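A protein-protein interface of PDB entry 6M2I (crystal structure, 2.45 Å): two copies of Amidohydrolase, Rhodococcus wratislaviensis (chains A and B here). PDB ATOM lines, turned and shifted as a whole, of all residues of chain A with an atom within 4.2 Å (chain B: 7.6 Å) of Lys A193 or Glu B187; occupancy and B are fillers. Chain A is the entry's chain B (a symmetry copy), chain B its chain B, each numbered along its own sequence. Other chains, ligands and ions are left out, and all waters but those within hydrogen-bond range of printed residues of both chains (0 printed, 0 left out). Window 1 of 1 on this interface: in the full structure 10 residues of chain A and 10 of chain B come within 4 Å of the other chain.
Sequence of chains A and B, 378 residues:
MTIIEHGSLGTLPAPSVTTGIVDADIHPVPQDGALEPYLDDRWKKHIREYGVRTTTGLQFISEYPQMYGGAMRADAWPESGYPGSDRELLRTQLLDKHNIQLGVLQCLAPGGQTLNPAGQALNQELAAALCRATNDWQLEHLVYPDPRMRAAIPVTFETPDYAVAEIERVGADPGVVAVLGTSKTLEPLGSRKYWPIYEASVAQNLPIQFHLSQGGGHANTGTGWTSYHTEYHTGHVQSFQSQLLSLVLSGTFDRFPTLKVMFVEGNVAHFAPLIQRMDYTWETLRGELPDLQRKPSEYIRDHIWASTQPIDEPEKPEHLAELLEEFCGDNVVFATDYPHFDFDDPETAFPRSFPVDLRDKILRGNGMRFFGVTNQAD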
ATOM      1  N   GLU A 158       7.807 -22.430   2.237  1.00  0.00           N
ATOM      2  CA  GLU A 158       9.214 -22.122   2.458  1.00  0.00           C
ATOM      3  C   GLU A 158       9.487 -20.636   2.651  1.00  0.00           C
ATOM      4  O   GLU A 158      10.615 -20.281   3.009  1.00  0.00           O
ATOM      5  CB  GLU A 158      10.076 -22.665   1.314  1.00  0.00           C
ATOM      6  CG  GLU A 158       9.837 -24.157   1.012  1.00  0.00           C
ATOM      7  CD  GLU A 158      10.184 -25.121   2.174  1.00  0.00           C
ATOM      8  OE1 GLU A 158      10.595 -24.678   3.281  1.00  0.00           O
ATOM      9  OE2 GLU A 158      10.063 -26.350   1.958  1.00  0.00           O
ATOM     10  N   PRO A 160       7.523 -18.258   4.976  1.00  0.00           N
ATOM     11  CA  PRO A 160       6.355 -18.070   5.865  1.00  0.00           C
ATOM     12  C   PRO A 160       5.697 -16.701   5.766  1.00  0.00           C
ATOM     13  O   PRO A 160       4.466 -16.619   5.856  1.00  0.00           O
ATOM     14  CB  PRO A 160       6.945 -18.324   7.258  1.00  0.00           C
ATOM     15  CG  PRO A 160       8.046 -19.344   6.984  1.00  0.00           C
ATOM     16  CD  PRO A 160       8.597 -19.035   5.614  1.00  0.00           C
ATOM     17  N   GLU A 187      13.060 -28.161   5.726  1.00  0.00           N
ATOM     18  CA  GLU A 187      13.193 -28.615   7.095  1.00  0.00           C
ATOM     19  C   GLU A 187      11.954 -29.409   7.464  1.00  0.00           C
ATOM     20  O   GLU A 187      10.897 -29.252   6.843  1.00  0.00           O
ATOM     21  CB  GLU A 187      13.359 -27.434   8.064  1.00  0.00           C
ATOM     22  CG  GLU A 187      14.122 -26.285   7.489  1.00  0.00           C
ATOM     23  CD  GLU A 187      14.514 -25.235   8.539  1.00  0.00           C
ATOM     24  OE1 GLU A 187      14.366 -25.500   9.751  1.00  0.00           O
ATOM     25  OE2 GLU A 187      14.965 -24.130   8.147  1.00  0.00           O
ATOM     26  N   SER A 191       9.714 -28.002  12.594  1.00  0.00           N
ATOM     27  CA  SER A 191      10.679 -26.935  12.787  1.00  0.00           C
ATOM     28  C   SER A 191       9.987 -25.586  12.975  1.00  0.00           C
ATOM     29  O   SER A 191       8.970 -25.292  12.348  1.00  0.00           O
ATOM     30  CB  SER A 191      11.613 -26.889  11.588  1.00  0.00           C
ATOM     31  OG  SER A 191      12.186 -25.603  11.449  1.00  0.00           O
ATOM     32  N   ARG A 192      10.566 -24.755  13.842  1.00  0.00           N
ATOM     33  CA  ARG A 192      10.045 -23.431  14.128  1.00  0.00           C
ATOM     34  C   ARG A 192       9.887 -22.562  12.881  1.00  0.00           C
ATOM     35  O   ARG A 192       9.112 -21.592  12.901  1.00  0.00           O
ATOM     36  CB  ARG A 192      10.970 -22.759  15.125  1.00  0.00           C
ATOM     37  CG  ARG A 192      10.283 -21.787  16.046  1.00  0.00           C
ATOM     38  CD  ARG A 192      11.274 -21.053  16.935  1.00  0.00           C
ATOM     39  NE  ARG A 192      10.641 -19.856  17.480  1.00  0.00           N
ATOM     40  CZ  ARG A 192      10.019 -19.811  18.656  1.00  0.00           C
ATOM     41  NH1 ARG A 192       9.456 -18.676  19.053  1.00  0.00           N
ATOM     42  NH2 ARG A 192       9.968 -20.896  19.432  1.00  0.00           N
ATOM     43  N   LYS A 193      10.581 -22.891  11.784  1.00  0.00           N
ATOM     44  CA  LYS A 193      10.462 -22.079  10.577  1.00  0.00           C
ATOM     45  C   LYS A 193       9.013 -21.930  10.142  1.00  0.00           C
ATOM     46  O   LYS A 193       8.640 -20.894   9.576  1.00  0.00           O
ATOM     47  CB  LYS A 193      11.297 -22.681   9.443  1.00  0.00           C
ATOM     48  CG  LYS A 193      10.942 -22.174   8.039  1.00  0.00           C
ATOM     49  CD  LYS A 193      11.974 -22.643   7.037  1.00  0.00           C
ATOM     50  CE  LYS A 193      11.444 -22.600   5.617  1.00  0.00           C
ATOM     51  NZ  LYS A 193      12.198 -21.622   4.819  1.00  0.00           N
ATOM     52  N   TYR A 194       8.184 -22.939  10.414  1.00  0.00           N
ATOM     53  CA  TYR A 194       6.809 -22.998   9.937  1.00  0.00           C
ATOM     54  C   TYR A 194       5.783 -22.573  10.979  1.00  0.00           C
ATOM     55  O   TYR A 194       4.611 -22.401  10.629  1.00  0.00           O
ATOM     56  CB  TYR A 194       6.479 -24.425   9.454  1.00  0.00           C
ATOM     57  CG  TYR A 194       7.488 -24.932   8.456  1.00  0.00           C
ATOM     58  CD1 TYR A 194       7.600 -24.348   7.198  1.00  0.00           C
ATOM     59  CD2 TYR A 194       8.343 -25.981   8.774  1.00  0.00           C
ATOM     60  CE1 TYR A 194       8.543 -24.791   6.288  1.00  0.00           C
ATOM     61  CE2 TYR A 194       9.278 -26.444   7.874  1.00  0.00           C
ATOM     62  CZ  TYR A 194       9.381 -25.843   6.633  1.00  0.00           C
ATOM     63  OH  TYR A 194      10.325 -26.294   5.735  1.00  0.00           O
ATOM     64  N   TRP A 195       6.187 -22.402  12.236  1.00  0.00           N
ATOM     65  CA  TRP A 195       5.245 -21.993  13.278  1.00  0.00           C
ATOM     66  C   TRP A 195       4.483 -20.711  12.958  1.00  0.00           C
ATOM     67  O   TRP A 195       3.304 -20.628  13.323  1.00  0.00           O
ATOM     68  CB  TRP A 195       5.983 -21.863  14.623  1.00  0.00           C
ATOM     69  CG  TRP A 195       6.323 -23.203  15.251  1.00  0.00           C
ATOM     70  CD1 TRP A 195       6.422 -24.407  14.612  1.00  0.00           C
ATOM     71  CD2 TRP A 195       6.607 -23.461  16.636  1.00  0.00           C
ATOM     72  NE1 TRP A 195       6.754 -25.393  15.508  1.00  0.00           N
ATOM     73  CE2 TRP A 195       6.879 -24.844  16.755  1.00  0.00           C
ATOM     74  CE3 TRP A 195       6.662 -22.660  17.787  1.00  0.00           C
ATOM     75  CZ2 TRP A 195       7.189 -25.449  17.985  1.00  0.00           C
ATOM     76  CZ3 TRP A 195       6.972 -23.262  19.014  1.00  0.00           C
ATOM     77  CH2 TRP A 195       7.222 -24.642  19.103  1.00  0.00           C
ATOM     78  N   PRO A 196       5.048 -19.702  12.292  1.00  0.00           N
ATOM     79  CA  PRO A 196       4.196 -18.566  11.903  1.00  0.00           C
ATOM     80  C   PRO A 196       3.046 -18.973  11.005  1.00  0.00           C
ATOM     81  O   PRO A 196       1.948 -18.402  11.115  1.00  0.00           O
ATOM     82  CB  PRO A 196       5.182 -17.615  11.198  1.00  0.00           C
ATOM     83  CG  PRO A 196       6.508 -17.923  11.830  1.00  0.00           C
ATOM     84  CD  PRO A 196       6.480 -19.422  12.025  1.00  0.00           C
ATOM     85  N   GLU B 158      20.148 -20.465  12.222  1.00  0.00           N
ATOM     86  CA  GLU B 158      19.085 -21.302  11.679  1.00  0.00           C
ATOM     87  C   GLU B 158      17.778 -21.199  12.453  1.00  0.00           C
ATOM     88  O   GLU B 158      16.767 -21.734  11.985  1.00  0.00           O
ATOM     89  CB  GLU B 158      19.529 -22.767  11.603  1.00  0.00           C
ATOM     90  CG  GLU B 158      20.872 -22.969  10.874  1.00  0.00           C
ATOM     91  CD  GLU B 158      20.875 -22.545   9.385  1.00  0.00           C
ATOM     92  OE1 GLU B 158      19.849 -22.040   8.853  1.00  0.00           O
ATOM     93  OE2 GLU B 158      21.928 -22.744   8.731  1.00  0.00           O
ATOM     94  N   THR B 159      17.760 -20.515  13.600  1.00  0.00           N
ATOM     95  CA  THR B 159      16.523 -20.200  14.323  1.00  0.00           C
ATOM     96  C   THR B 159      16.465 -18.698  14.569  1.00  0.00           C
ATOM     97  O   THR B 159      16.806 -18.221  15.661  1.00  0.00           O
ATOM     98  CB  THR B 159      16.441 -20.957  15.644  1.00  0.00           C
ATOM     99  OG1 THR B 159      16.763 -22.329  15.414  1.00  0.00           O
ATOM    100  CG2 THR B 159      15.045 -20.849  16.229  1.00  0.00           C
ATOM    101  N   PRO B 160      16.059 -17.924  13.566  1.00  0.00           N
ATOM    102  CA  PRO B 160      16.147 -16.451  13.687  1.00  0.00           C
ATOM    103  C   PRO B 160      15.543 -15.883  14.963  1.00  0.00           C
ATOM    104  O   PRO B 160      16.093 -14.919  15.510  1.00  0.00           O
ATOM    105  CB  PRO B 160      15.404 -15.964  12.435  1.00  0.00           C
ATOM    106  CG  PRO B 160      15.685 -17.067  11.419  1.00  0.00           C
ATOM    107  CD  PRO B 160      15.775 -18.360  12.190  1.00  0.00           C
ATOM    108  N   ASP B 161      14.455 -16.472  15.473  1.00  0.00           N
ATOM    109  CA  ASP B 161      13.822 -15.963  16.688  1.00  0.00           C
ATOM    110  C   ASP B 161      14.801 -15.927  17.850  1.00  0.00           C
ATOM    111  O   ASP B 161      14.888 -14.928  18.573  1.00  0.00           O
ATOM    112  CB  ASP B 161      12.614 -16.827  17.057  1.00  0.00           C
ATOM    113  CG  ASP B 161      11.352 -16.372  16.376  1.00  0.00           C
ATOM    114  OD1 ASP B 161      11.369 -15.266  15.799  1.00  0.00           O
ATOM    115  OD2 ASP B 161      10.344 -17.115  16.422  1.00  0.00           O
ATOM    116  N   SER B 183      29.856 -19.902   7.616  1.00  0.00           N
ATOM    117  CA  SER B 183      29.792 -19.851   6.152  1.00  0.00           C
ATOM    118  C   SER B 183      28.787 -20.840   5.589  1.00  0.00           C
ATOM    119  O   SER B 183      28.241 -20.608   4.509  1.00  0.00           O
ATOM    120  CB  SER B 183      31.164 -20.125   5.536  1.00  0.00           C
ATOM    121  OG  SER B 183      31.606 -21.420   5.901  1.00  0.00           O
ATOM    122  N   LYS B 184      28.524 -21.937   6.288  1.00  0.00           N
ATOM    123  CA  LYS B 184      27.618 -22.966   5.790  1.00  0.00           C
ATOM    124  C   LYS B 184      26.267 -22.849   6.478  1.00  0.00           C
ATOM    125  O   LYS B 184      26.189 -22.764   7.711  1.00  0.00           O
ATOM    126  CB  LYS B 184      28.226 -24.358   5.976  1.00  0.00           C
ATOM    127  CG  LYS B 184      29.490 -24.523   5.124  1.00  0.00           C
ATOM    128  CD  LYS B 184      29.944 -25.947   5.016  1.00  0.00           C
ATOM    129  CE  LYS B 184      30.785 -26.154   3.759  1.00  0.00           C
ATOM    130  NZ  LYS B 184      32.160 -25.600   3.921  1.00  0.00           N
ATOM    131  N   THR B 185      25.209 -22.820   5.672  1.00  0.00           N
ATOM    132  CA  THR B 185      23.859 -22.602   6.149  1.00  0.00           C
ATOM    133  C   THR B 185      22.899 -23.505   5.380  1.00  0.00           C
ATOM    134  O   THR B 185      23.246 -24.096   4.350  1.00  0.00           O
ATOM    135  CB  THR B 185      23.449 -21.128   5.995  1.00  0.00           C
ATOM    136  OG1 THR B 185      23.691 -20.706   4.642  1.00  0.00           O
ATOM    137  CG2 THR B 185      24.227 -20.240   6.970  1.00  0.00           C
ATOM    138  N   LEU B 186      21.673 -23.601   5.894  1.00  0.00           N
ATOM    139  CA  LEU B 186      20.687 -24.481   5.281  1.00  0.00           C
ATOM    140  C   LEU B 186      20.177 -23.887   3.987  1.00  0.00           C
ATOM    141  O   LEU B 186      19.965 -24.610   3.004  1.00  0.00           O
ATOM    142  CB  LEU B 186      19.538 -24.741   6.252  1.00  0.00           C
ATOM    143  CG  LEU B 186      19.871 -25.786   7.332  1.00  0.00           C
ATOM    144  CD1 LEU B 186      18.974 -25.684   8.589  1.00  0.00           C
ATOM    145  CD2 LEU B 186      19.859 -27.206   6.739  1.00  0.00           C
ATOM    146  N   GLU B 187      19.999 -22.573   3.966  1.00  0.00           N
ATOM    147  CA  GLU B 187      19.654 -21.793   2.795  1.00  0.00           C
ATOM    148  C   GLU B 187      20.721 -20.734   2.587  1.00  0.00           C
ATOM    149  O   GLU B 187      21.438 -20.371   3.525  1.00  0.00           O
ATOM    150  CB  GLU B 187      18.280 -21.121   2.953  1.00  0.00           C
ATOM    151  CG  GLU B 187      17.298 -21.932   3.733  1.00  0.00           C
ATOM    152  CD  GLU B 187      15.865 -21.385   3.655  1.00  0.00           C
ATOM    153  OE1 GLU B 187      15.601 -20.487   2.828  1.00  0.00           O
ATOM    154  OE2 GLU B 187      14.999 -21.850   4.436  1.00  0.00           O
ATOM    155  N   PRO B 188      20.863 -20.220   1.375  1.00  0.00           N
ATOM    156  CA  PRO B 188      21.873 -19.181   1.152  1.00  0.00           C
ATOM    157  C   PRO B 188      21.529 -17.918   1.935  1.00  0.00           C
ATOM    158  O   PRO B 188      20.363 -17.571   2.115  1.00  0.00           O
ATOM    159  CB  PRO B 188      21.826 -18.964  -0.364  1.00  0.00           C
ATOM    160  CG  PRO B 188      21.221 -20.262  -0.925  1.00  0.00           C
ATOM    161  CD  PRO B 188      20.244 -20.696   0.123  1.00  0.00           C
ATOM    162  N   LEU B 189      22.562 -17.231   2.411  1.00  0.00           N
ATOM    163  CA  LEU B 189      22.355 -16.146   3.367  1.00  0.00           C
ATOM    164  C   LEU B 189      21.498 -15.000   2.836  1.00  0.00           C
ATOM    165  O   LEU B 189      21.054 -14.165   3.631  1.00  0.00           O
ATOM    166  CB  LEU B 189      23.691 -15.606   3.826  1.00  0.00           C
ATOM    167  CG  LEU B 189      24.374 -16.503   4.845  1.00  0.00           C
ATOM    168  CD1 LEU B 189      25.839 -16.085   4.980  1.00  0.00           C
ATOM    169  CD2 LEU B 189      23.600 -16.385   6.159  1.00  0.00           C
ATOM    170  N   GLY B 190      21.272 -14.912   1.528  1.00  0.00           N
ATOM    171  CA  GLY B 190      20.371 -13.876   1.048  1.00  0.00           C
ATOM    172  C   GLY B 190      18.903 -14.213   1.195  1.00  0.00           C
ATOM    173  O   GLY B 190      18.041 -13.339   1.039  1.00  0.00           O
ATOM    174  N   SER B 191      18.615 -15.468   1.515  1.00  0.00           N
ATOM    175  CA  SER B 191      17.247 -15.915   1.699  1.00  0.00           C
ATOM    176  C   SER B 191      16.549 -15.131   2.809  1.00  0.00           C
ATOM    177  O   SER B 191      17.149 -14.783   3.825  1.00  0.00           O
ATOM    178  CB  SER B 191      17.250 -17.401   2.023  1.00  0.00           C
ATOM    179  OG  SER B 191      16.076 -17.764   2.723  1.00  0.00           O
ATOM    180  N   ARG B 192      15.257 -14.868   2.607  1.00  0.00           N
ATOM    181  CA  ARG B 192      14.444 -14.144   3.567  1.00  0.00           C
ATOM    182  C   ARG B 192      14.447 -14.775   4.959  1.00  0.00           C
ATOM    183  O   ARG B 192      14.143 -14.087   5.947  1.00  0.00           O
ATOM    184  CB  ARG B 192      13.028 -14.062   3.028  1.00  0.00           C
ATOM    185  CG  ARG B 192      12.279 -12.827   3.449  1.00  0.00           C
ATOM    186  CD  ARG B 192      10.831 -12.859   2.987  1.00  0.00           C
ATOM    187  NE  ARG B 192      10.055 -11.893   3.758  1.00  0.00           N
ATOM    188  CZ  ARG B 192       9.831 -10.639   3.372  1.00  0.00           C
ATOM    189  NH1 ARG B 192       9.129  -9.830   4.156  1.00  0.00           N
ATOM    190  NH2 ARG B 192      10.303 -10.200   2.203  1.00  0.00           N
ATOM    191  N   LYS B 193      14.805 -16.059   5.074  1.00  0.00           N
ATOM    192  CA  LYS B 193      14.810 -16.699   6.386  1.00  0.00           C
ATOM    193  C   LYS B 193      15.659 -15.924   7.383  1.00  0.00           C
ATOM    194  O   LYS B 193      15.353 -15.919   8.582  1.00  0.00           O
ATOM    195  CB  LYS B 193      15.309 -18.143   6.276  1.00  0.00           C
ATOM    196  CG  LYS B 193      15.747 -18.779   7.601  1.00  0.00           C
ATOM    197  CD  LYS B 193      15.987 -20.261   7.417  1.00  0.00           C
ATOM    198  CE  LYS B 193      16.861 -20.835   8.514  1.00  0.00           C
ATOM    199  NZ  LYS B 193      16.107 -21.811   9.313  1.00  0.00           N
ATOM    200  N   TYR B 194      16.708 -15.254   6.904  1.00  0.00           N
ATOM    201  CA  TYR B 194      17.687 -14.586   7.752  1.00  0.00           C
ATOM    202  C   TYR B 194      17.459 -13.086   7.881  1.00  0.00           C
ATOM    203  O   TYR B 194      18.108 -12.453   8.721  1.00  0.00           O
ATOM    204  CB  TYR B 194      19.109 -14.838   7.214  1.00  0.00           C
ATOM    205  CG  TYR B 194      19.387 -16.306   7.011  1.00  0.00           C
ATOM    206  CD1 TYR B 194      19.458 -17.173   8.097  1.00  0.00           C
ATOM    207  CD2 TYR B 194      19.558 -16.830   5.735  1.00  0.00           C
ATOM    208  CE1 TYR B 194      19.686 -18.525   7.915  1.00  0.00           C
ATOM    209  CE2 TYR B 194      19.797 -18.174   5.538  1.00  0.00           C
ATOM    210  CZ  TYR B 194      19.854 -19.021   6.629  1.00  0.00           C
ATOM    211  OH  TYR B 194      20.080 -20.367   6.434  1.00  0.00           O
ATOM    212  N   TYR B 198      19.240  -9.858  10.169  1.00  0.00           N
ATOM    213  CA  TYR B 198      19.845  -8.635   9.674  1.00  0.00           C
ATOM    214  C   TYR B 198      19.110  -7.423  10.231  1.00  0.00           C
ATOM    215  O   TYR B 198      19.734  -6.459  10.678  1.00  0.00           O
ATOM    216  CB  TYR B 198      19.851  -8.617   8.142  1.00  0.00           C
ATOM    217  CG  TYR B 198      20.440  -9.857   7.504  1.00  0.00           C
ATOM    218  CD1 TYR B 198      21.462 -10.583   8.129  1.00  0.00           C
ATOM    219  CD2 TYR B 198      20.000 -10.287   6.257  1.00  0.00           C
ATOM    220  CE1 TYR B 198      22.017 -11.725   7.527  1.00  0.00           C
ATOM    221  CE2 TYR B 198      20.541 -11.416   5.645  1.00  0.00           C
ATOM    222  CZ  TYR B 198      21.538 -12.143   6.288  1.00  0.00           C
ATOM    223  OH  TYR B 198      22.045 -13.274   5.676  1.00  0.00           O
ATOM    224  N   GLY B 216      26.148 -27.136   8.280  1.00  0.00           N
ATOM    225  CA  GLY B 216      25.184 -26.332   7.577  1.00  0.00           C
ATOM    226  C   GLY B 216      24.008 -27.106   7.021  1.00  0.00           C
ATOM    227  O   GLY B 216      22.953 -26.512   6.787  1.00  0.00           O
ATOM    228  N   HIS B 218      24.164 -29.354   4.129  1.00  0.00           N
ATOM    229  CA  HIS B 218      24.462 -29.941   2.828  1.00  0.00           C
ATOM    230  C   HIS B 218      25.920 -30.386   2.791  1.00  0.00           C
ATOM    231  O   HIS B 218      26.694 -30.132   3.720  1.00  0.00           O
ATOM    232  CB  HIS B 218      24.165 -28.955   1.687  1.00  0.00           C
ATOM    233  CG  HIS B 218      22.893 -28.176   1.867  1.00  0.00           C
ATOM    234  ND1 HIS B 218      21.679 -28.600   1.363  1.00  0.00           N
ATOM    235  CD2 HIS B 218      22.652 -26.998   2.494  1.00  0.00           C
ATOM    236  CE1 HIS B 218      20.746 -27.716   1.669  1.00  0.00           C
ATOM    237  NE2 HIS B 218      21.310 -26.734   2.353  1.00  0.00           N
ATOM    238  N   GLN B 243      27.641 -17.664  -0.895  1.00  0.00           N
ATOM    239  CA  GLN B 243      27.002 -16.719   0.015  1.00  0.00           C
ATOM    240  C   GLN B 243      27.103 -15.284  -0.502  1.00  0.00           C
ATOM    241  O   GLN B 243      26.171 -14.497  -0.316  1.00  0.00           O
ATOM    242  CB  GLN B 243      27.608 -16.841   1.414  1.00  0.00           C
ATOM    243  CG  GLN B 243      27.466 -18.231   2.049  1.00  0.00           C
ATOM    244  CD  GLN B 243      26.042 -18.553   2.549  1.00  0.00           C
ATOM    245  OE1 GLN B 243      25.040 -18.036   2.035  1.00  0.00           O
ATOM    246  NE2 GLN B 243      25.958 -19.413   3.569  1.00  0.00           N
ATOM    247  N   SER B 246      24.351 -15.031  -3.327  1.00  0.00           N
ATOM    248  CA  SER B 246      23.036 -14.936  -2.710  1.00  0.00           C
ATOM    249  C   SER B 246      22.822 -13.568  -2.061  1.00  0.00           C
ATOM    250  O   SER B 246      21.823 -12.891  -2.331  1.00  0.00           O
ATOM    251  CB  SER B 246      22.861 -16.036  -1.677  1.00  0.00           C
ATOM    252  OG  SER B 246      21.509 -16.075  -1.236  1.00  0.00           O
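Glu A187 touches Lys B193, and with the chains exchanged Lys A193 touches Glu B187.
Of the 4 pairs that touch across the chains among the printed residues, 2 have their exchanged pair printed and touching as well.
OG1 of Thr B185 sits at hydrogen-bond distance from O of Glu B187.
The side-chain hydroxyl (OG) of Ser B191 lies within hydrogen-bond range of the side-chain carboxylate (OE1) of Glu B187.
The backbone carbonyl oxygen of Glu B187 sits at hydrogen-bond distance from the side-chain hydroxyl of Tyr B194.
The side-chain hydroxyl (OG) of Ser B191 sits close to the backbone NH (N) of Lys B193 (3.2 Å).
OE1 of Glu A158 is in salt-bridge range of NZ of Lys A193, at 3.8 Å.
The backbone carbonyl oxygen (O) of Glu A187 lies within hydrogen-bond range of the side-chain hydroxyl (OH) of Tyr A194 (3.2 Å).
Of the 21 printed residues of chain B, 4 touch a printed residue of chain A.
Printed residues of chain B that touch a printed residue of chain A: Thr B159, Asp B161, Glu B187 and Lys B193.
Of the 9 printed residues of chain A, 3 touch a printed residue of chain B.
Among the printed residues, 4 pairs touch across the chains.
Among the printed residues, Asp or Glu carboxylates within 4 Å of a Lys or Arg side-chain nitrogen of the other chain: Glu A187 with Lys B193 (2.8 Å), Arg A192 with Asp B161 (3.0 Å) and Lys A193 with Glu B187 (2.8 Å).
Among the printed residues, merely in contact across the chains: Arg A192 with Thr B159.
The side-chain carboxylate (OD2) of Asp B161 is in salt-bridge range of the guanidinium group (NE) of Arg A192 (3.0 Å).
NZ of Lys A193 is in salt-bridge range of OE2 of Glu B187 (2.8 Å).
The side-chain carboxylate (OE2) of Glu A187 lies within salt-bridge range of the side-chain amino group (NZ) of Lys B193 (2.8 Å).
Of the printed residues of chain B, Arg A192 touches Thr B159 and Asp B161.
Lys A193 touches one residue of chain B.
Of the printed residues of chain A, Thr B159 touches Arg A192.
Of the printed residues of chain A, Asp B161 touches Arg A192.
Glu B187 touches just one residue of chain A: Lys A193.
Of the printed residues of chain A, Lys B193 touches Glu A187 (2.8 Å).
The nearest printed residue of chain A that does not touch Glu B187 is Glu A187 (4.4 Å).
The nearest printed residue of chain A that does not touch Thr B159 is Lys A193 (6.6 Å).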
